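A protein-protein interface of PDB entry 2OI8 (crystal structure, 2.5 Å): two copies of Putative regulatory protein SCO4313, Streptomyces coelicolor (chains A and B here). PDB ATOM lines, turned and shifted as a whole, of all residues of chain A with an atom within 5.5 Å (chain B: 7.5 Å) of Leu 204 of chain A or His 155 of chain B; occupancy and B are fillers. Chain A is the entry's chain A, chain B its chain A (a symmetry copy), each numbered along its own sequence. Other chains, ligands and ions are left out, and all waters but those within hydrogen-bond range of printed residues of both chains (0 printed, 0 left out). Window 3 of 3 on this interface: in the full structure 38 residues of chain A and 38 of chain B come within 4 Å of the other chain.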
ATOM      1  N   GLY A 199      12.160 -13.991  -0.817  1.00  0.00           N
ATOM      2  CA  GLY A 199      12.068 -13.214  -2.061  1.00  0.00           C
ATOM      3  C   GLY A 199      12.295 -13.931  -3.383  1.00  0.00           C
ATOM      4  O   GLY A 199      12.208 -13.317  -4.446  1.00  0.00           O
ATOM      5  N   PHE A 200      12.605 -15.220  -3.333  1.00  0.00           N
ATOM      6  CA  PHE A 200      12.605 -16.027  -4.544  1.00  0.00           C
ATOM      7  C   PHE A 200      11.236 -16.692  -4.705  1.00  0.00           C
ATOM      8  O   PHE A 200      10.365 -16.564  -3.836  1.00  0.00           O
ATOM      9  CB  PHE A 200      13.754 -17.046  -4.558  1.00  0.00           C
ATOM     10  CG  PHE A 200      13.618 -18.152  -3.541  1.00  0.00           C
ATOM     11  CD1 PHE A 200      12.876 -19.300  -3.827  1.00  0.00           C
ATOM     12  CD2 PHE A 200      14.258 -18.067  -2.314  1.00  0.00           C
ATOM     13  CE1 PHE A 200      12.758 -20.321  -2.890  1.00  0.00           C
ATOM     14  CE2 PHE A 200      14.146 -19.089  -1.376  1.00  0.00           C
ATOM     15  CZ  PHE A 200      13.400 -20.210  -1.663  1.00  0.00           C
ATOM     16  N   ASP A 201      11.063 -17.390  -5.823  1.00  0.00           N
ATOM     17  CA  ASP A 201       9.801 -17.981  -6.179  1.00  0.00           C
ATOM     18  C   ASP A 201       9.893 -19.463  -5.899  1.00  0.00           C
ATOM     19  O   ASP A 201      10.374 -20.248  -6.726  1.00  0.00           O
ATOM     20  CB  ASP A 201       9.511 -17.706  -7.645  1.00  0.00           C
ATOM     21  CG  ASP A 201       8.130 -18.144  -8.072  1.00  0.00           C
ATOM     22  OD1 ASP A 201       7.367 -18.707  -7.265  1.00  0.00           O
ATOM     23  OD2 ASP A 201       7.806 -17.927  -9.252  1.00  0.00           O
ATOM     24  N   SER A 202       9.430 -19.835  -4.704  1.00  0.00           N
ATOM     25  CA  SER A 202       9.437 -21.219  -4.230  1.00  0.00           C
ATOM     26  C   SER A 202       8.756 -22.201  -5.195  1.00  0.00           C
ATOM     27  O   SER A 202       9.137 -23.363  -5.240  1.00  0.00           O
ATOM     28  CB  SER A 202       8.790 -21.311  -2.846  1.00  0.00           C
ATOM     29  OG  SER A 202       7.384 -21.135  -2.929  1.00  0.00           O
ATOM     30  N   ALA A 203       7.769 -21.735  -5.962  1.00  0.00           N
ATOM     31  CA  ALA A 203       7.169 -22.554  -7.013  1.00  0.00           C
ATOM     32  C   ALA A 203       8.224 -23.020  -8.033  1.00  0.00           C
ATOM     33  O   ALA A 203       8.124 -24.120  -8.586  1.00  0.00           O
ATOM     34  CB  ALA A 203       6.054 -21.795  -7.706  1.00  0.00           C
ATOM     35  N   LEU A 204       9.233 -22.184  -8.268  1.00  0.00           N
ATOM     36  CA  LEU A 204      10.312 -22.514  -9.212  1.00  0.00           C
ATOM     37  C   LEU A 204      11.268 -23.487  -8.557  1.00  0.00           C
ATOM     38  O   LEU A 204      11.688 -24.454  -9.195  1.00  0.00           O
ATOM     39  CB  LEU A 204      11.052 -21.263  -9.705  1.00  0.00           C
ATOM     40  CG  LEU A 204      10.557 -20.492 -10.940  1.00  0.00           C
ATOM     41  CD1 LEU A 204       9.047 -20.562 -11.165  1.00  0.00           C
ATOM     42  CD2 LEU A 204      11.026 -19.028 -10.896  1.00  0.00           C
ATOM     43  N   LEU A 205      11.582 -23.236  -7.279  1.00  0.00           N
ATOM     44  CA  LEU A 205      12.264 -24.239  -6.442  1.00  0.00           C
ATOM     45  C   LEU A 205      11.599 -25.623  -6.545  1.00  0.00           C
ATOM     46  O   LEU A 205      12.276 -26.624  -6.789  1.00  0.00           O
ATOM     47  CB  LEU A 205      12.379 -23.795  -4.977  1.00  0.00           C
ATOM     48  CG  LEU A 205      12.859 -24.913  -4.037  1.00  0.00           C
ATOM     49  CD1 LEU A 205      14.238 -25.480  -4.405  1.00  0.00           C
ATOM     50  CD2 LEU A 205      12.819 -24.489  -2.574  1.00  0.00           C
ATOM     51  N   PHE A 206      10.281 -25.654  -6.397  1.00  0.00           N
ATOM     52  CA  PHE A 206       9.509 -26.881  -6.506  1.00  0.00           C
ATOM     53  C   PHE A 206       9.709 -27.514  -7.875  1.00  0.00           C
ATOM     54  O   PHE A 206       9.967 -28.721  -7.958  1.00  0.00           O
ATOM     55  CB  PHE A 206       8.020 -26.591  -6.245  1.00  0.00           C
ATOM     56  CG  PHE A 206       7.139 -27.814  -6.286  1.00  0.00           C
ATOM     57  CD1 PHE A 206       6.719 -28.357  -7.506  1.00  0.00           C
ATOM     58  CD2 PHE A 206       6.706 -28.411  -5.107  1.00  0.00           C
ATOM     59  CE1 PHE A 206       5.879 -29.492  -7.542  1.00  0.00           C
ATOM     60  CE2 PHE A 206       5.871 -29.563  -5.132  1.00  0.00           C
ATOM     61  CZ  PHE A 206       5.455 -30.095  -6.351  1.00  0.00           C
ATOM     62  N   GLU A 207       9.589 -26.705  -8.937  1.00  0.00           N
ATOM     63  CA  GLU A 207       9.890 -27.158 -10.307  1.00  0.00           C
ATOM     64  C   GLU A 207      11.294 -27.727 -10.453  1.00  0.00           C
ATOM     65  O   GLU A 207      11.479 -28.746 -11.139  1.00  0.00           O
ATOM     66  CB  GLU A 207       9.733 -26.041 -11.355  1.00  0.00           C
ATOM     67  CG  GLU A 207       8.324 -25.730 -11.788  1.00  0.00           C
ATOM     68  CD  GLU A 207       7.504 -26.967 -12.053  1.00  0.00           C
ATOM     69  OE1 GLU A 207       7.699 -27.630 -13.101  1.00  0.00           O
ATOM     70  OE2 GLU A 207       6.651 -27.268 -11.196  1.00  0.00           O
ATOM     71  N   ALA A 208      12.274 -27.042  -9.860  1.00  0.00           N
ATOM     72  CA  ALA A 208      13.655 -27.492  -9.924  1.00  0.00           C
ATOM     73  C   ALA A 208      13.787 -28.865  -9.257  1.00  0.00           C
ATOM     74  O   ALA A 208      14.320 -29.799  -9.861  1.00  0.00           O
ATOM     75  CB  ALA A 208      14.578 -26.491  -9.286  1.00  0.00           C
ATOM     76  N   GLU A 209      13.272 -28.997  -8.036  1.00  0.00           N
ATOM     77  CA  GLU A 209      13.368 -30.254  -7.295  1.00  0.00           C
ATOM     78  C   GLU A 209      12.699 -31.410  -8.016  1.00  0.00           C
ATOM     79  O   GLU A 209      13.207 -32.522  -8.004  1.00  0.00           O
ATOM     80  CB  GLU A 209      12.804 -30.098  -5.884  1.00  0.00           C
ATOM     81  CG  GLU A 209      13.753 -29.390  -4.942  1.00  0.00           C
ATOM     82  CD  GLU A 209      15.006 -30.194  -4.685  1.00  0.00           C
ATOM     83  OE1 GLU A 209      14.949 -31.144  -3.886  1.00  0.00           O
ATOM     84  OE2 GLU A 209      16.059 -29.894  -5.285  1.00  0.00           O
ATOM     85  N   GLY B 150      20.943 -24.027 -15.757  1.00  0.00           N
ATOM     86  CA  GLY B 150      19.662 -24.458 -15.189  1.00  0.00           C
ATOM     87  C   GLY B 150      18.747 -23.290 -14.877  1.00  0.00           C
ATOM     88  O   GLY B 150      19.193 -22.245 -14.391  1.00  0.00           O
ATOM     89  N   ALA B 151      17.456 -23.484 -15.127  1.00  0.00           N
ATOM     90  CA  ALA B 151      16.462 -22.416 -15.013  1.00  0.00           C
ATOM     91  C   ALA B 151      16.268 -21.751 -13.625  1.00  0.00           C
ATOM     92  O   ALA B 151      15.989 -20.544 -13.559  1.00  0.00           O
ATOM     93  CB  ALA B 151      15.120 -22.900 -15.563  1.00  0.00           C
ATOM     94  N   PHE B 152      16.402 -22.508 -12.534  1.00  0.00           N
ATOM     95  CA  PHE B 152      16.226 -21.916 -11.204  1.00  0.00           C
ATOM     96  C   PHE B 152      17.386 -21.016 -10.793  1.00  0.00           C
ATOM     97  O   PHE B 152      17.156 -19.926 -10.230  1.00  0.00           O
ATOM     98  CB  PHE B 152      15.953 -22.985 -10.149  1.00  0.00           C
ATOM     99  CG  PHE B 152      15.566 -22.429  -8.795  1.00  0.00           C
ATOM    100  CD1 PHE B 152      14.568 -21.446  -8.674  1.00  0.00           C
ATOM    101  CD2 PHE B 152      16.177 -22.914  -7.625  1.00  0.00           C
ATOM    102  CE1 PHE B 152      14.200 -20.943  -7.407  1.00  0.00           C
ATOM    103  CE2 PHE B 152      15.814 -22.417  -6.349  1.00  0.00           C
ATOM    104  CZ  PHE B 152      14.827 -21.434  -6.246  1.00  0.00           C
ATOM    105  N   ASP B 153      18.620 -21.465 -11.082  1.00  0.00           N
ATOM    106  CA  ASP B 153      19.834 -20.652 -10.906  1.00  0.00           C
ATOM    107  C   ASP B 153      19.674 -19.275 -11.566  1.00  0.00           C
ATOM    108  O   ASP B 153      19.954 -18.246 -10.946  1.00  0.00           O
ATOM    109  CB  ASP B 153      21.089 -21.349 -11.474  1.00  0.00           C
ATOM    110  CG  ASP B 153      21.225 -22.807 -11.016  1.00  0.00           C
ATOM    111  OD1 ASP B 153      20.918 -23.125  -9.847  1.00  0.00           O
ATOM    112  OD2 ASP B 153      21.658 -23.642 -11.837  1.00  0.00           O
ATOM    113  N   ALA B 154      19.210 -19.258 -12.816  1.00  0.00           N
ATOM    114  CA  ALA B 154      18.972 -18.000 -13.541  1.00  0.00           C
ATOM    115  C   ALA B 154      18.062 -17.055 -12.755  1.00  0.00           C
ATOM    116  O   ALA B 154      18.332 -15.851 -12.665  1.00  0.00           O
ATOM    117  CB  ALA B 154      18.372 -18.277 -14.910  1.00  0.00           C
ATOM    118  N   HIS B 155      16.988 -17.612 -12.203  1.00  0.00           N
ATOM    119  CA  HIS B 155      16.087 -16.861 -11.349  1.00  0.00           C
ATOM    120  C   HIS B 155      16.808 -16.299 -10.123  1.00  0.00           C
ATOM    121  O   HIS B 155      16.608 -15.148  -9.748  1.00  0.00           O
ATOM    122  CB  HIS B 155      14.945 -17.770 -10.921  1.00  0.00           C
ATOM    123  CG  HIS B 155      14.065 -17.189  -9.862  1.00  0.00           C
ATOM    124  ND1 HIS B 155      13.125 -16.216 -10.127  1.00  0.00           N
ATOM    125  CD2 HIS B 155      13.964 -17.466  -8.538  1.00  0.00           C
ATOM    126  CE1 HIS B 155      12.480 -15.921  -9.011  1.00  0.00           C
ATOM    127  NE2 HIS B 155      12.975 -16.659  -8.032  1.00  0.00           N
ATOM    128  N   LEU B 156      17.658 -17.122  -9.519  1.00  0.00           N
ATOM    129  CA  LEU B 156      18.315 -16.791  -8.256  1.00  0.00           C
ATOM    130  C   LEU B 156      19.314 -15.636  -8.346  1.00  0.00           C
ATOM    131  O   LEU B 156      19.654 -15.025  -7.324  1.00  0.00           O
ATOM    132  CB  LEU B 156      19.020 -18.030  -7.703  1.00  0.00           C
ATOM    133  CG  LEU B 156      18.342 -18.906  -6.641  1.00  0.00           C
ATOM    134  CD1 LEU B 156      16.834 -18.874  -6.737  1.00  0.00           C
ATOM    135  CD2 LEU B 156      18.853 -20.333  -6.725  1.00  0.00           C
ATOM    136  N   ASP B 157      19.783 -15.345  -9.557  1.00  0.00           N
ATOM    137  CA  ASP B 157      20.765 -14.277  -9.777  1.00  0.00           C
ATOM    138  C   ASP B 157      20.151 -12.915  -9.521  1.00  0.00           C
ATOM    139  O   ASP B 157      20.824 -11.996  -9.060  1.00  0.00           O
ATOM    140  CB  ASP B 157      21.322 -14.324 -11.207  1.00  0.00           C
ATOM    141  CG  ASP B 157      22.415 -15.359 -11.374  1.00  0.00           C
ATOM    142  OD1 ASP B 157      23.567 -14.962 -11.687  1.00  0.00           O
ATOM    143  OD2 ASP B 157      22.135 -16.571 -11.184  1.00  0.00           O
ATOM    144  N   THR B 158      18.867 -12.796  -9.835  1.00  0.00           N
ATOM    145  CA  THR B 158      18.110 -11.583  -9.564  1.00  0.00           C
ATOM    146  C   THR B 158      17.340 -11.682  -8.217  1.00  0.00           C
ATOM    147  O   THR B 158      16.832 -10.680  -7.705  1.00  0.00           O
ATOM    148  CB  THR B 158      17.214 -11.181 -10.804  1.00  0.00           C
ATOM    149  OG1 THR B 158      16.555  -9.934 -10.562  1.00  0.00           O
ATOM    150  CG2 THR B 158      16.177 -12.267 -11.157  1.00  0.00           C
ATOM    151  N   HIS B 159      17.308 -12.883  -7.631  1.00  0.00           N
ATOM    152  CA  HIS B 159      16.531 -13.148  -6.412  1.00  0.00           C
ATOM    153  C   HIS B 159      17.345 -13.806  -5.287  1.00  0.00           C
ATOM    154  O   HIS B 159      17.233 -15.012  -5.043  1.00  0.00           O
ATOM    155  CB  HIS B 159      15.306 -14.000  -6.753  1.00  0.00           C
ATOM    156  CG  HIS B 159      14.279 -13.277  -7.564  1.00  0.00           C
ATOM    157  ND1 HIS B 159      14.192 -13.397  -8.936  1.00  0.00           N
ATOM    158  CD2 HIS B 159      13.299 -12.413  -7.200  1.00  0.00           C
ATOM    159  CE1 HIS B 159      13.203 -12.643  -9.382  1.00  0.00           C
ATOM    160  NE2 HIS B 159      12.646 -12.031  -8.350  1.00  0.00           N
ATOM    161  N   ARG B 160      18.148 -13.008  -4.585  1.00  0.00           N
ATOM    162  CA  ARG B 160      19.107 -13.565  -3.624  1.00  0.00           C
ATOM    163  C   ARG B 160      19.387 -12.688  -2.410  1.00  0.00           C
ATOM    164  O   ARG B 160      20.263 -13.021  -1.598  1.00  0.00           O
ATOM    165  CB  ARG B 160      20.420 -13.900  -4.323  1.00  0.00           C
ATOM    166  CG  ARG B 160      21.082 -12.699  -4.978  1.00  0.00           C
ATOM    167  CD  ARG B 160      22.138 -13.160  -5.940  1.00  0.00           C
ATOM    168  NE  ARG B 160      23.332 -13.641  -5.246  1.00  0.00           N
ATOM    169  CZ  ARG B 160      24.124 -14.609  -5.701  1.00  0.00           C
ATOM    170  NH1 ARG B 160      23.846 -15.234  -6.842  1.00  0.00           N
ATOM    171  NH2 ARG B 160      25.193 -14.967  -5.005  1.00  0.00           N
ATOM    172  N   SER B 170      25.022 -18.648  -8.216  1.00  0.00           N
ATOM    173  CA  SER B 170      23.675 -18.983  -7.816  1.00  0.00           C
ATOM    174  C   SER B 170      23.426 -20.482  -7.701  1.00  0.00           C
ATOM    175  O   SER B 170      22.501 -20.890  -6.998  1.00  0.00           O
ATOM    176  CB  SER B 170      22.663 -18.342  -8.757  1.00  0.00           C
ATOM    177  OG  SER B 170      22.498 -16.961  -8.452  1.00  0.00           O
ATOM    178  N   HIS B 174      21.238 -22.465  -5.000  1.00  0.00           N
ATOM    179  CA  HIS B 174      20.301 -23.501  -5.415  1.00  0.00           C
ATOM    180  C   HIS B 174      20.562 -24.806  -4.646  1.00  0.00           C
ATOM    181  O   HIS B 174      19.640 -25.406  -4.066  1.00  0.00           O
ATOM    182  CB  HIS B 174      20.435 -23.736  -6.915  1.00  0.00           C
ATOM    183  CG  HIS B 174      19.467 -24.738  -7.463  1.00  0.00           C
ATOM    184  ND1 HIS B 174      18.674 -25.530  -6.659  1.00  0.00           N
ATOM    185  CD2 HIS B 174      19.199 -25.111  -8.736  1.00  0.00           C
ATOM    186  CE1 HIS B 174      17.951 -26.338  -7.413  1.00  0.00           C
ATOM    187  NE2 HIS B 174      18.254 -26.104  -8.677  1.00  0.00           N
ATOM    188  N   LEU B 177      19.430 -24.365  -0.921  1.00  0.00           N
ATOM    189  CA  LEU B 177      17.976 -24.478  -0.814  1.00  0.00           C
ATOM    190  C   LEU B 177      17.517 -25.938  -0.936  1.00  0.00           C
ATOM    191  O   LEU B 177      16.660 -26.357  -0.193  1.00  0.00           O
ATOM    192  CB  LEU B 177      17.306 -23.586  -1.873  1.00  0.00           C
ATOM    193  CG  LEU B 177      17.541 -22.077  -1.725  1.00  0.00           C
ATOM    194  CD1 LEU B 177      16.973 -21.343  -2.893  1.00  0.00           C
ATOM    195  CD2 LEU B 177      16.924 -21.559  -0.444  1.00  0.00           C
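Of the 11 printed residues of chain A, 6 touch a printed residue of chain B.
Hydrophobic or aromatic side chains of chain A within 4 Å of the printed part of chain B: Phe 200, Leu 204, Leu 205 and Ala 208.
Hydrophobic or aromatic side chains of chain B that line the printed part of chain A: Phe 152, His 155, His 159, His 174 and Leu 177.
No position is printed for both chains.
N of Asp 201 of chain A lies within hydrogen-bond range of NE2 of His 155 of chain B (3.0 Å).
Among the printed residues, pairs that only touch across the chains: Gly 199 of chain A with His 159 of chain B (3.1 Å), Phe 200 of chain A with Phe 152 of chain B (3.8 Å), Phe 200 of chain A with His 155 of chain B (3.6 Å), Phe 200 of chain A with Leu 177 of chain B (3.8 Å), Asp 201 of chain A with Phe 152 of chain B (3.9 Å), Leu 204 of chain A with Phe 152 of chain B (3.7 Å), Leu 204 of chain A with His 155 of chain B (3.6 Å), Leu 205 of chain A with Phe 152 of chain B (3.5 Å), Ala 208 of chain A with Phe 152 of chain B (3.9 Å) and Ala 208 of chain A with His 174 of chain B (3.7 Å).
Of chain B, only Phe 152 (3.7 Å) and His 155 (3.6 Å) come within 4 Å of Leu 204 of chain A.
His 155 of chain B touches three residues of chain A.
No residue of chain B comes within 4 Å of Ala 203 of chain A.
Of the printed residues of chain A, His 174 of chain B touches Ala 208 (3.7 Å).
Of the printed residues of chain A, Phe 152 of chain B touches Phe 200, Asp 201, Leu 204, Leu 205 and Ala 208.
Printed residues of chain B within 4 Å of Leu 205 of chain A: Phe 152.
Phe 206 of chain A touches none of the printed residues of chain B.
Gly 150 of chain B touches none of the printed residues of chain A.
The nearest residue of chain A that does not touch His 155 of chain B is Gly 199 of chain A (5.0 Å).
The side-chain carboxylate of Asp 201 of chain A lies close to the backbone NH of Ala 203 of chain A, 3.3 Å away.
A ring nitrogen (ND1) of His 159 of chain B lies close to the backbone carbonyl oxygen of His 155 of chain B.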
